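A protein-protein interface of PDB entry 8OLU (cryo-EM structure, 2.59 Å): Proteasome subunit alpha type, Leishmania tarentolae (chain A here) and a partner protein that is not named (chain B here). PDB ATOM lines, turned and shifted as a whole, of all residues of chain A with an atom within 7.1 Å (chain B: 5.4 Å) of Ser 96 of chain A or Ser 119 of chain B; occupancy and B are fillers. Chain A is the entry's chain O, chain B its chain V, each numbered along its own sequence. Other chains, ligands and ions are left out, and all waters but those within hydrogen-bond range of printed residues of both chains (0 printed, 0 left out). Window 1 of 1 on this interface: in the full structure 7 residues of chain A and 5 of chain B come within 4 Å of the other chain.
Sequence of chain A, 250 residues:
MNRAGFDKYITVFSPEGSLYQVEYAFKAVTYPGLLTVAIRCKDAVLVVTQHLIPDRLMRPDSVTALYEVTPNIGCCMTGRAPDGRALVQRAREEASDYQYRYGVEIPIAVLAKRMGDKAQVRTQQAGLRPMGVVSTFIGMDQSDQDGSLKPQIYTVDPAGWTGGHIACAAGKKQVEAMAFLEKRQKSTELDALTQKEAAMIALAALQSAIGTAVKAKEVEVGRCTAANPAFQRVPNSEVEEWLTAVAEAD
Of the 11 printed residues of chain B, 4 touch a printed residue of chain A. Printed residues of chain B that touch a printed residue of chain A: Asn 115, Ser 119, Thr 122 and Asp 123. Of the 19 printed residues of chain A, 7 touch a printed residue of chain B. Printed residues of chain A that touch a printed residue of chain B: Glu 68, Val 69, Gln 89, Arg 92, Ser 96, Gln 99 and Tyr 100. Among the printed residues, 9 pairs touch across the chains. Among the printed residues, Asp or Glu carboxylates within 4 Å of a Lys or Arg side-chain nitrogen of the other chain: Arg 92 of chain A with Asp 123 of chain B.
Of chain B, only Asn 115 and Ser 119 come within 4 Å of Ser 96 of chain A. Of the printed residues of chain B, Gln 99 of chain A touches Asn 115. Of the printed residues of chain B, Tyr 100 of chain A touches Asn 115. Arg 101 of chain A touches none of the printed residues of chain B. Of the printed residues of chain A, Ser 119 of chain B touches Ser 96. The nearest printed residue of chain B that does not touch Ser 96 of chain A is Gly 118 of chain B (6.6 Å). The nearest residue of chain A that does not touch Ser 119 of chain B is Arg 92 of chain A (4.7 Å).
The side-chain carboxylate (OE2) of Glu 68 of chain A sits at hydrogen-bond distance from the side-chain hydroxyl (OG1) of Thr 122 of chain B, 2.9 Å away. NE2 of Gln 89 of chain A lies within hydrogen-bond range of OD1 of Asp 123 of chain B (2.9 Å). The guanidinium group (NH1) of Arg 92 of chain A lies within salt-bridge range of the side-chain carboxylate (OD1) of Asp 123 of chain B (3.5 Å). The side-chain amide nitrogen (ND2) of Asn 115 of chain B is in hydrogen-bond range of the backbone carbonyl oxygen (O) of Ser 96 of chain A (3.2 Å). The backbone NH of Tyr 100 of chain A lies close to the side-chain amide nitrogen of Asn 115 of chain B (3.5 Å).
O of Glu 68 of chain A is in hydrogen-bond range of NH2 of Arg 92 of chain A (2.6 Å). The backbone carbonyl oxygen of Arg 92 of chain A lies within hydrogen-bond range of the side-chain hydroxyl of Ser 96 of chain A (3.3 Å). O of Glu 93 of chain A sits at hydrogen-bond distance from OG of Ser 96 of chain A, 3.1 Å away. O of Gly 118 of chain B lies within hydrogen-bond range of OG1 of Thr 122 of chain B.
Among the printed residues, merely in contact across the chains: Ser 96 of chain A with Ser 119 of chain B, Gln 99 of chain A with Asn 115 of chain B, Arg 92 of chain A with Thr 122 of chain B and Val 69 of chain A with Thr 122 of chain B.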
ATOM      1  N   GLU A  68       6.050  12.743   1.005  1.00  0.00           N
ATOM      2  CA  GLU A  68       6.539  11.525   1.581  1.00  0.00           C
ATOM      3  C   GLU A  68       7.154  10.753   0.417  1.00  0.00           C
ATOM      4  O   GLU A  68       6.651  10.774  -0.707  1.00  0.00           O
ATOM      5  CB  GLU A  68       5.406  10.951   2.417  1.00  0.00           C
ATOM      6  CG  GLU A  68       5.427   9.449   2.598  1.00  0.00           C
ATOM      7  CD  GLU A  68       4.125   8.846   3.149  1.00  0.00           C
ATOM      8  OE1 GLU A  68       3.483   9.504   4.024  1.00  0.00           O
ATOM      9  OE2 GLU A  68       3.750   7.707   2.718  1.00  0.00           O
ATOM     10  N   VAL A  69       8.361  10.260   0.651  1.00  0.00           N
ATOM     11  CA  VAL A  69       9.005   9.374  -0.277  1.00  0.00           C
ATOM     12  C   VAL A  69       8.757   7.955   0.173  1.00  0.00           C
ATOM     13  O   VAL A  69       8.437   7.099  -0.608  1.00  0.00           O
ATOM     14  CB  VAL A  69      10.508   9.643  -0.328  1.00  0.00           C
ATOM     15  CG1 VAL A  69      11.249   8.550  -1.036  1.00  0.00           C
ATOM     16  CG2 VAL A  69      10.740  10.955  -1.015  1.00  0.00           C
ATOM     17  N   THR A  70       9.087   7.703   1.410  1.00  0.00           N
ATOM     18  CA  THR A  70       8.584   6.568   2.110  1.00  0.00           C
ATOM     19  C   THR A  70       8.022   7.093   3.412  1.00  0.00           C
ATOM     20  O   THR A  70       8.314   8.223   3.779  1.00  0.00           O
ATOM     21  CB  THR A  70       9.694   5.541   2.374  1.00  0.00           C
ATOM     22  OG1 THR A  70      10.674   5.857   3.370  1.00  0.00           O
ATOM     23  CG2 THR A  70      10.452   5.256   1.105  1.00  0.00           C
ATOM     24  N   GLN A  89       8.520  10.855  -7.866  1.00  0.00           N
ATOM     25  CA  GLN A  89       8.164   9.574  -8.414  1.00  0.00           C
ATOM     26  C   GLN A  89       9.367   8.634  -8.525  1.00  0.00           C
ATOM     27  O   GLN A  89       9.263   7.460  -8.265  1.00  0.00           O
ATOM     28  CB  GLN A  89       7.534   9.767  -9.782  1.00  0.00           C
ATOM     29  CG  GLN A  89       6.018  10.024  -9.808  1.00  0.00           C
ATOM     30  CD  GLN A  89       5.243   9.967  -8.496  1.00  0.00           C
ATOM     31  OE1 GLN A  89       4.852  11.019  -7.968  1.00  0.00           O
ATOM     32  NE2 GLN A  89       5.002   8.769  -7.957  1.00  0.00           N
ATOM     33  N   ARG A  90      10.494   9.108  -9.005  1.00  0.00           N
ATOM     34  CA  ARG A  90      11.623   8.247  -9.232  1.00  0.00           C
ATOM     35  C   ARG A  90      12.164   7.827  -7.897  1.00  0.00           C
ATOM     36  O   ARG A  90      12.674   6.732  -7.801  1.00  0.00           O
ATOM     37  CB  ARG A  90      12.812   8.897  -9.960  1.00  0.00           C
ATOM     38  CG  ARG A  90      12.574   9.398 -11.376  1.00  0.00           C
ATOM     39  CD  ARG A  90      12.455   8.325 -12.429  1.00  0.00           C
ATOM     40  NE  ARG A  90      11.083   7.774 -12.523  1.00  0.00           N
ATOM     41  CZ  ARG A  90       9.948   8.462 -12.791  1.00  0.00           C
ATOM     42  NH1 ARG A  90       8.789   7.810 -12.800  1.00  0.00           N
ATOM     43  NH2 ARG A  90       9.963   9.774 -13.044  1.00  0.00           N
ATOM     44  N   ALA A  91      12.218   8.731  -6.952  1.00  0.00           N
ATOM     45  CA  ALA A  91      12.670   8.383  -5.623  1.00  0.00           C
ATOM     46  C   ALA A  91      11.855   7.251  -5.027  1.00  0.00           C
ATOM     47  O   ALA A  91      12.352   6.455  -4.275  1.00  0.00           O
ATOM     48  CB  ALA A  91      12.491   9.579  -4.729  1.00  0.00           C
ATOM     49  N   ARG A  92      10.557   7.359  -5.246  1.00  0.00           N
ATOM     50  CA  ARG A  92       9.563   6.476  -4.698  1.00  0.00           C
ATOM     51  C   ARG A  92       9.701   5.077  -5.232  1.00  0.00           C
ATOM     52  O   ARG A  92       9.512   4.121  -4.470  1.00  0.00           O
ATOM     53  CB  ARG A  92       8.194   7.028  -5.027  1.00  0.00           C
ATOM     54  CG  ARG A  92       7.697   7.875  -3.877  1.00  0.00           C
ATOM     55  CD  ARG A  92       6.496   8.636  -4.361  1.00  0.00           C
ATOM     56  NE  ARG A  92       6.047   9.449  -3.292  1.00  0.00           N
ATOM     57  CZ  ARG A  92       5.033  10.216  -3.446  1.00  0.00           C
ATOM     58  NH1 ARG A  92       4.372  10.169  -4.587  1.00  0.00           N
ATOM     59  NH2 ARG A  92       4.766  11.069  -2.491  1.00  0.00           N
ATOM     60  N   GLU A  93       9.913   5.044  -6.539  1.00  0.00           N
ATOM     61  CA  GLU A  93      10.237   3.847  -7.243  1.00  0.00           C
ATOM     62  C   GLU A  93      11.540   3.283  -6.727  1.00  0.00           C
ATOM     63  O   GLU A  93      11.717   2.081  -6.751  1.00  0.00           O
ATOM     64  CB  GLU A  93      10.584   4.054  -8.703  1.00  0.00           C
ATOM     65  CG  GLU A  93       9.443   4.223  -9.684  1.00  0.00           C
ATOM     66  CD  GLU A  93      10.046   4.407 -11.094  1.00  0.00           C
ATOM     67  OE1 GLU A  93       9.799   5.488 -11.734  1.00  0.00           O
ATOM     68  OE2 GLU A  93      10.824   3.486 -11.544  1.00  0.00           O
ATOM     69  N   GLU A  94      12.492   4.139  -6.451  1.00  0.00           N
ATOM     70  CA  GLU A  94      13.780   3.650  -6.067  1.00  0.00           C
ATOM     71  C   GLU A  94      13.655   3.035  -4.688  1.00  0.00           C
ATOM     72  O   GLU A  94      14.214   2.016  -4.379  1.00  0.00           O
ATOM     73  CB  GLU A  94      14.798   4.775  -6.051  1.00  0.00           C
ATOM     74  CG  GLU A  94      16.189   4.288  -5.824  1.00  0.00           C
ATOM     75  CD  GLU A  94      16.752   3.409  -6.956  1.00  0.00           C
ATOM     76  OE1 GLU A  94      17.492   2.370  -6.657  1.00  0.00           O
ATOM     77  OE2 GLU A  94      16.397   3.706  -8.154  1.00  0.00           O
ATOM     78  N   ALA A  95      12.914   3.691  -3.860  1.00  0.00           N
ATOM     79  CA  ALA A  95      12.730   3.293  -2.502  1.00  0.00           C
ATOM     80  C   ALA A  95      11.959   1.994  -2.442  1.00  0.00           C
ATOM     81  O   ALA A  95      12.130   1.252  -1.496  1.00  0.00           O
ATOM     82  CB  ALA A  95      11.925   4.386  -1.815  1.00  0.00           C
ATOM     83  N   SER A  96      10.991   1.856  -3.322  1.00  0.00           N
ATOM     84  CA  SER A  96      10.158   0.688  -3.315  1.00  0.00           C
ATOM     85  C   SER A  96      10.876  -0.483  -3.940  1.00  0.00           C
ATOM     86  O   SER A  96      10.704  -1.572  -3.425  1.00  0.00           O
ATOM     87  CB  SER A  96       8.880   0.896  -4.030  1.00  0.00           C
ATOM     88  OG  SER A  96       9.097   1.037  -5.428  1.00  0.00           O
ATOM     89  N   ASP A  97      11.643  -0.279  -5.008  1.00  0.00           N
ATOM     90  CA  ASP A  97      12.431  -1.340  -5.569  1.00  0.00           C
ATOM     91  C   ASP A  97      13.421  -1.770  -4.532  1.00  0.00           C
ATOM     92  O   ASP A  97      13.640  -2.956  -4.397  1.00  0.00           O
ATOM     93  CB  ASP A  97      13.232  -0.999  -6.805  1.00  0.00           C
ATOM     94  CG  ASP A  97      12.432  -0.525  -8.037  1.00  0.00           C
ATOM     95  OD1 ASP A  97      11.147  -0.661  -8.070  1.00  0.00           O
ATOM     96  OD2 ASP A  97      13.085   0.055  -8.979  1.00  0.00           O
ATOM     97  N   TYR A  98      13.923  -0.852  -3.742  1.00  0.00           N
ATOM     98  CA  TYR A  98      14.910  -1.209  -2.766  1.00  0.00           C
ATOM     99  C   TYR A  98      14.305  -2.025  -1.671  1.00  0.00           C
ATOM    100  O   TYR A  98      14.961  -2.926  -1.207  1.00  0.00           O
ATOM    101  CB  TYR A  98      15.560   0.041  -2.177  1.00  0.00           C
ATOM    102  CG  TYR A  98      16.634  -0.155  -1.152  1.00  0.00           C
ATOM    103  CD1 TYR A  98      17.961  -0.068  -1.459  1.00  0.00           C
ATOM    104  CD2 TYR A  98      16.314  -0.518   0.136  1.00  0.00           C
ATOM    105  CE1 TYR A  98      18.919  -0.199  -0.477  1.00  0.00           C
ATOM    106  CE2 TYR A  98      17.264  -0.773   1.088  1.00  0.00           C
ATOM    107  CZ  TYR A  98      18.576  -0.542   0.804  1.00  0.00           C
ATOM    108  OH  TYR A  98      19.480  -0.739   1.861  1.00  0.00           O
ATOM    109  N   GLN A  99      13.093  -1.720  -1.229  1.00  0.00           N
ATOM    110  CA  GLN A  99      12.468  -2.487  -0.147  1.00  0.00           C
ATOM    111  C   GLN A  99      12.171  -3.911  -0.631  1.00  0.00           C
ATOM    112  O   GLN A  99      12.341  -4.906   0.090  1.00  0.00           O
ATOM    113  CB  GLN A  99      11.270  -1.693   0.352  1.00  0.00           C
ATOM    114  CG  GLN A  99      10.064  -2.476   0.875  1.00  0.00           C
ATOM    115  CD  GLN A  99      10.278  -2.925   2.291  1.00  0.00           C
ATOM    116  OE1 GLN A  99      10.560  -2.104   3.163  1.00  0.00           O
ATOM    117  NE2 GLN A  99      10.139  -4.235   2.502  1.00  0.00           N
ATOM    118  N   TYR A 100      11.779  -4.006  -1.903  1.00  0.00           N
ATOM    119  CA  TYR A 100      11.518  -5.308  -2.438  1.00  0.00           C
ATOM    120  C   TYR A 100      12.797  -6.124  -2.484  1.00  0.00           C
ATOM    121  O   TYR A 100      12.789  -7.278  -2.130  1.00  0.00           O
ATOM    122  CB  TYR A 100      10.776  -5.219  -3.766  1.00  0.00           C
ATOM    123  CG  TYR A 100      10.355  -6.571  -4.281  1.00  0.00           C
ATOM    124  CD1 TYR A 100       9.366  -7.280  -3.625  1.00  0.00           C
ATOM    125  CD2 TYR A 100      11.026  -7.204  -5.323  1.00  0.00           C
ATOM    126  CE1 TYR A 100       9.026  -8.578  -4.000  1.00  0.00           C
ATOM    127  CE2 TYR A 100      10.688  -8.495  -5.722  1.00  0.00           C
ATOM    128  CZ  TYR A 100       9.671  -9.189  -5.069  1.00  0.00           C
ATOM    129  OH  TYR A 100       9.261 -10.468  -5.409  1.00  0.00           O
ATOM    130  N   ARG A 101      13.895  -5.545  -2.908  1.00  0.00           N
ATOM    131  CA  ARG A 101      15.109  -6.288  -3.109  1.00  0.00           C
ATOM    132  C   ARG A 101      15.723  -6.624  -1.766  1.00  0.00           C
ATOM    133  O   ARG A 101      16.198  -7.708  -1.601  1.00  0.00           O
ATOM    134  CB  ARG A 101      16.026  -5.520  -4.049  1.00  0.00           C
ATOM    135  CG  ARG A 101      17.406  -6.133  -4.186  1.00  0.00           C
ATOM    136  CD  ARG A 101      18.487  -5.409  -5.026  1.00  0.00           C
ATOM    137  NE  ARG A 101      18.336  -5.543  -6.474  1.00  0.00           N
ATOM    138  CZ  ARG A 101      17.325  -5.032  -7.177  1.00  0.00           C
ATOM    139  NH1 ARG A 101      16.631  -3.993  -6.728  1.00  0.00           N
ATOM    140  NH2 ARG A 101      17.025  -5.562  -8.349  1.00  0.00           N
ATOM    141  N   TYR A 102      15.711  -5.766  -0.779  1.00  0.00           N
ATOM    142  CA  TYR A 102      16.483  -6.029   0.411  1.00  0.00           C
ATOM    143  C   TYR A 102      15.602  -6.287   1.632  1.00  0.00           C
ATOM    144  O   TYR A 102      16.067  -6.466   2.726  1.00  0.00           O
ATOM    145  CB  TYR A 102      17.405  -4.855   0.689  1.00  0.00           C
ATOM    146  CG  TYR A 102      18.418  -4.612  -0.391  1.00  0.00           C
ATOM    147  CD1 TYR A 102      19.534  -5.400  -0.531  1.00  0.00           C
ATOM    148  CD2 TYR A 102      18.255  -3.611  -1.327  1.00  0.00           C
ATOM    149  CE1 TYR A 102      20.455  -5.177  -1.544  1.00  0.00           C
ATOM    150  CE2 TYR A 102      19.169  -3.360  -2.335  1.00  0.00           C
ATOM    151  CZ  TYR A 102      20.273  -4.170  -2.470  1.00  0.00           C
ATOM    152  OH  TYR A 102      21.174  -3.956  -3.499  1.00  0.00           O
ATOM    153  N   VAL A 104      14.189  -4.202   3.446  1.00  0.00           N
ATOM    154  CA  VAL A 104      14.226  -3.140   4.438  1.00  0.00           C
ATOM    155  C   VAL A 104      13.982  -1.813   3.762  1.00  0.00           C
ATOM    156  O   VAL A 104      14.089  -1.672   2.576  1.00  0.00           O
ATOM    157  CB  VAL A 104      15.524  -3.122   5.252  1.00  0.00           C
ATOM    158  CG1 VAL A 104      15.793  -4.480   5.856  1.00  0.00           C
ATOM    159  CG2 VAL A 104      16.712  -2.733   4.425  1.00  0.00           C
ATOM    160  N   ILE A 106      14.703   1.809   2.637  1.00  0.00           N
ATOM    161  CA  ILE A 106      15.914   2.374   2.106  1.00  0.00           C
ATOM    162  C   ILE A 106      16.400   3.459   3.035  1.00  0.00           C
ATOM    163  O   ILE A 106      15.640   4.275   3.546  1.00  0.00           O
ATOM    164  CB  ILE A 106      15.693   2.903   0.696  1.00  0.00           C
ATOM    165  CG1 ILE A 106      17.005   3.347   0.084  1.00  0.00           C
ATOM    166  CG2 ILE A 106      14.667   4.025   0.613  1.00  0.00           C
ATOM    167  CD1 ILE A 106      16.879   3.493  -1.389  1.00  0.00           C
ATOM    168  N   SER B 114       2.532  -6.635  -0.480  1.00  0.00           N
ATOM    169  CA  SER B 114       2.707  -5.654   0.562  1.00  0.00           C
ATOM    170  C   SER B 114       3.524  -4.482   0.054  1.00  0.00           C
ATOM    171  O   SER B 114       3.354  -3.359   0.467  1.00  0.00           O
ATOM    172  CB  SER B 114       3.402  -6.285   1.680  1.00  0.00           C
ATOM    173  OG  SER B 114       3.523  -5.427   2.803  1.00  0.00           O
ATOM    174  N   ASN B 115       4.480  -4.792  -0.793  1.00  0.00           N
ATOM    175  CA  ASN B 115       5.331  -3.835  -1.422  1.00  0.00           C
ATOM    176  C   ASN B 115       4.479  -2.990  -2.294  1.00  0.00           C
ATOM    177  O   ASN B 115       4.551  -1.806  -2.151  1.00  0.00           O
ATOM    178  CB  ASN B 115       6.421  -4.468  -2.280  1.00  0.00           C
ATOM    179  CG  ASN B 115       7.479  -3.478  -2.737  1.00  0.00           C
ATOM    180  OD1 ASN B 115       7.409  -3.037  -3.900  1.00  0.00           O
ATOM    181  ND2 ASN B 115       8.399  -3.112  -1.830  1.00  0.00           N
ATOM    182  N   TYR B 116       3.725  -3.578  -3.204  1.00  0.00           N
ATOM    183  CA  TYR B 116       2.914  -2.760  -4.098  1.00  0.00           C
ATOM    184  C   TYR B 116       2.003  -1.839  -3.344  1.00  0.00           C
ATOM    185  O   TYR B 116       1.757  -0.788  -3.850  1.00  0.00           O
ATOM    186  CB  TYR B 116       1.986  -3.548  -5.016  1.00  0.00           C
ATOM    187  CG  TYR B 116       2.677  -4.247  -6.146  1.00  0.00           C
ATOM    188  CD1 TYR B 116       3.740  -3.653  -6.787  1.00  0.00           C
ATOM    189  CD2 TYR B 116       2.242  -5.484  -6.620  1.00  0.00           C
ATOM    190  CE1 TYR B 116       4.380  -4.280  -7.842  1.00  0.00           C
ATOM    191  CE2 TYR B 116       2.882  -6.146  -7.663  1.00  0.00           C
ATOM    192  CZ  TYR B 116       3.952  -5.521  -8.301  1.00  0.00           C
ATOM    193  OH  TYR B 116       4.665  -6.061  -9.375  1.00  0.00           O
ATOM    194  N   LEU B 117       1.443  -2.312  -2.249  1.00  0.00           N
ATOM    195  CA  LEU B 117       0.452  -1.587  -1.514  1.00  0.00           C
ATOM    196  C   LEU B 117       1.065  -0.468  -0.725  1.00  0.00           C
ATOM    197  O   LEU B 117       0.362   0.492  -0.472  1.00  0.00           O
ATOM    198  CB  LEU B 117      -0.222  -2.466  -0.481  1.00  0.00           C
ATOM    199  CG  LEU B 117      -1.270  -3.432  -1.010  1.00  0.00           C
ATOM    200  CD1 LEU B 117      -1.873  -4.147   0.178  1.00  0.00           C
ATOM    201  CD2 LEU B 117      -2.320  -2.689  -1.826  1.00  0.00           C
ATOM    202  N   GLY B 118       2.301  -0.627  -0.281  1.00  0.00           N
ATOM    203  CA  GLY B 118       2.968   0.473   0.383  1.00  0.00           C
ATOM    204  C   GLY B 118       3.295   1.591  -0.602  1.00  0.00           C
ATOM    205  O   GLY B 118       3.050   2.762  -0.311  1.00  0.00           O
ATOM    206  N   SER B 119       3.818   1.215  -1.777  1.00  0.00           N
ATOM    207  CA  SER B 119       3.994   2.154  -2.844  1.00  0.00           C
ATOM    208  C   SER B 119       2.691   2.881  -3.095  1.00  0.00           C
ATOM    209  O   SER B 119       2.682   4.083  -3.246  1.00  0.00           O
ATOM    210  CB  SER B 119       4.415   1.511  -4.093  1.00  0.00           C
ATOM    211  OG  SER B 119       5.794   1.239  -4.076  1.00  0.00           O
ATOM    212  N   TYR B 120       1.602   2.144  -3.207  1.00  0.00           N
ATOM    213  CA  TYR B 120       0.330   2.724  -3.574  1.00  0.00           C
ATOM    214  C   TYR B 120      -0.209   3.662  -2.497  1.00  0.00           C
ATOM    215  O   TYR B 120      -0.896   4.617  -2.776  1.00  0.00           O
ATOM    216  CB  TYR B 120      -0.675   1.610  -3.732  1.00  0.00           C
ATOM    217  CG  TYR B 120      -2.068   2.080  -4.074  1.00  0.00           C
ATOM    218  CD1 TYR B 120      -2.315   2.627  -5.306  1.00  0.00           C
ATOM    219  CD2 TYR B 120      -3.119   1.980  -3.181  1.00  0.00           C
ATOM    220  CE1 TYR B 120      -3.597   2.987  -5.666  1.00  0.00           C
ATOM    221  CE2 TYR B 120      -4.384   2.368  -3.511  1.00  0.00           C
ATOM    222  CZ  TYR B 120      -4.615   2.916  -4.749  1.00  0.00           C
ATOM    223  OH  TYR B 120      -5.826   3.351  -5.208  1.00  0.00           O
ATOM    224  N   GLN B 121       0.109   3.387  -1.252  1.00  0.00           N
ATOM    225  CA  GLN B 121      -0.409   4.210  -0.197  1.00  0.00           C
ATOM    226  C   GLN B 121       0.331   5.527  -0.127  1.00  0.00           C
ATOM    227  O   GLN B 121      -0.229   6.539   0.231  1.00  0.00           O
ATOM    228  CB  GLN B 121      -0.272   3.411   1.071  1.00  0.00           C
ATOM    229  CG  GLN B 121      -0.704   4.139   2.319  1.00  0.00           C
ATOM    230  CD  GLN B 121      -0.702   3.107   3.426  1.00  0.00           C
ATOM    231  OE1 GLN B 121      -0.400   1.924   3.218  1.00  0.00           O
ATOM    232  NE2 GLN B 121      -1.050   3.565   4.616  1.00  0.00           N
ATOM    233  N   THR B 122       1.624   5.462  -0.401  1.00  0.00           N
ATOM    234  CA  THR B 122       2.481   6.633  -0.420  1.00  0.00           C
ATOM    235  C   THR B 122       2.103   7.542  -1.584  1.00  0.00           C
ATOM    236  O   THR B 122       2.065   8.745  -1.449  1.00  0.00           O
ATOM    237  CB  THR B 122       3.924   6.145  -0.479  1.00  0.00           C
ATOM    238  OG1 THR B 122       4.307   5.641   0.805  1.00  0.00           O
ATOM    239  CG2 THR B 122       4.872   7.249  -0.839  1.00  0.00           C
ATOM    240  N   ASP B 123       1.669   6.929  -2.659  1.00  0.00           N
ATOM    241  CA  ASP B 123       1.307   7.635  -3.846  1.00  0.00           C
ATOM    242  C   ASP B 123      -0.059   8.314  -3.789  1.00  0.00           C
ATOM    243  O   ASP B 123      -0.248   9.366  -4.383  1.00  0.00           O
ATOM    244  CB  ASP B 123       1.248   6.680  -5.030  1.00  0.00           C
ATOM    245  CG  ASP B 123       1.479   7.435  -6.335  1.00  0.00           C
ATOM    246  OD1 ASP B 123       2.670   7.885  -6.560  1.00  0.00           O
ATOM    247  OD2 ASP B 123       0.465   7.644  -7.081  1.00  0.00           O
ATOM    248  N   ILE B 124      -1.064   7.673  -3.223  1.00  0.00           N
ATOM    249  CA  ILE B 124      -2.354   8.313  -3.180  1.00  0.00           C
ATOM    250  C   ILE B 124      -2.477   9.134  -1.898  1.00  0.00           C
ATOM    251  O   ILE B 124      -3.489   9.779  -1.678  1.00  0.00           O
ATOM    252  CB  ILE B 124      -3.469   7.258  -3.252  1.00  0.00           C
ATOM    253  CG1 ILE B 124      -3.625   6.567  -1.907  1.00  0.00           C
ATOM    254  CG2 ILE B 124      -3.258   6.259  -4.383  1.00  0.00           C
ATOM    255  CD1 ILE B 124      -4.452   5.351  -1.962  1.00  0.00           C
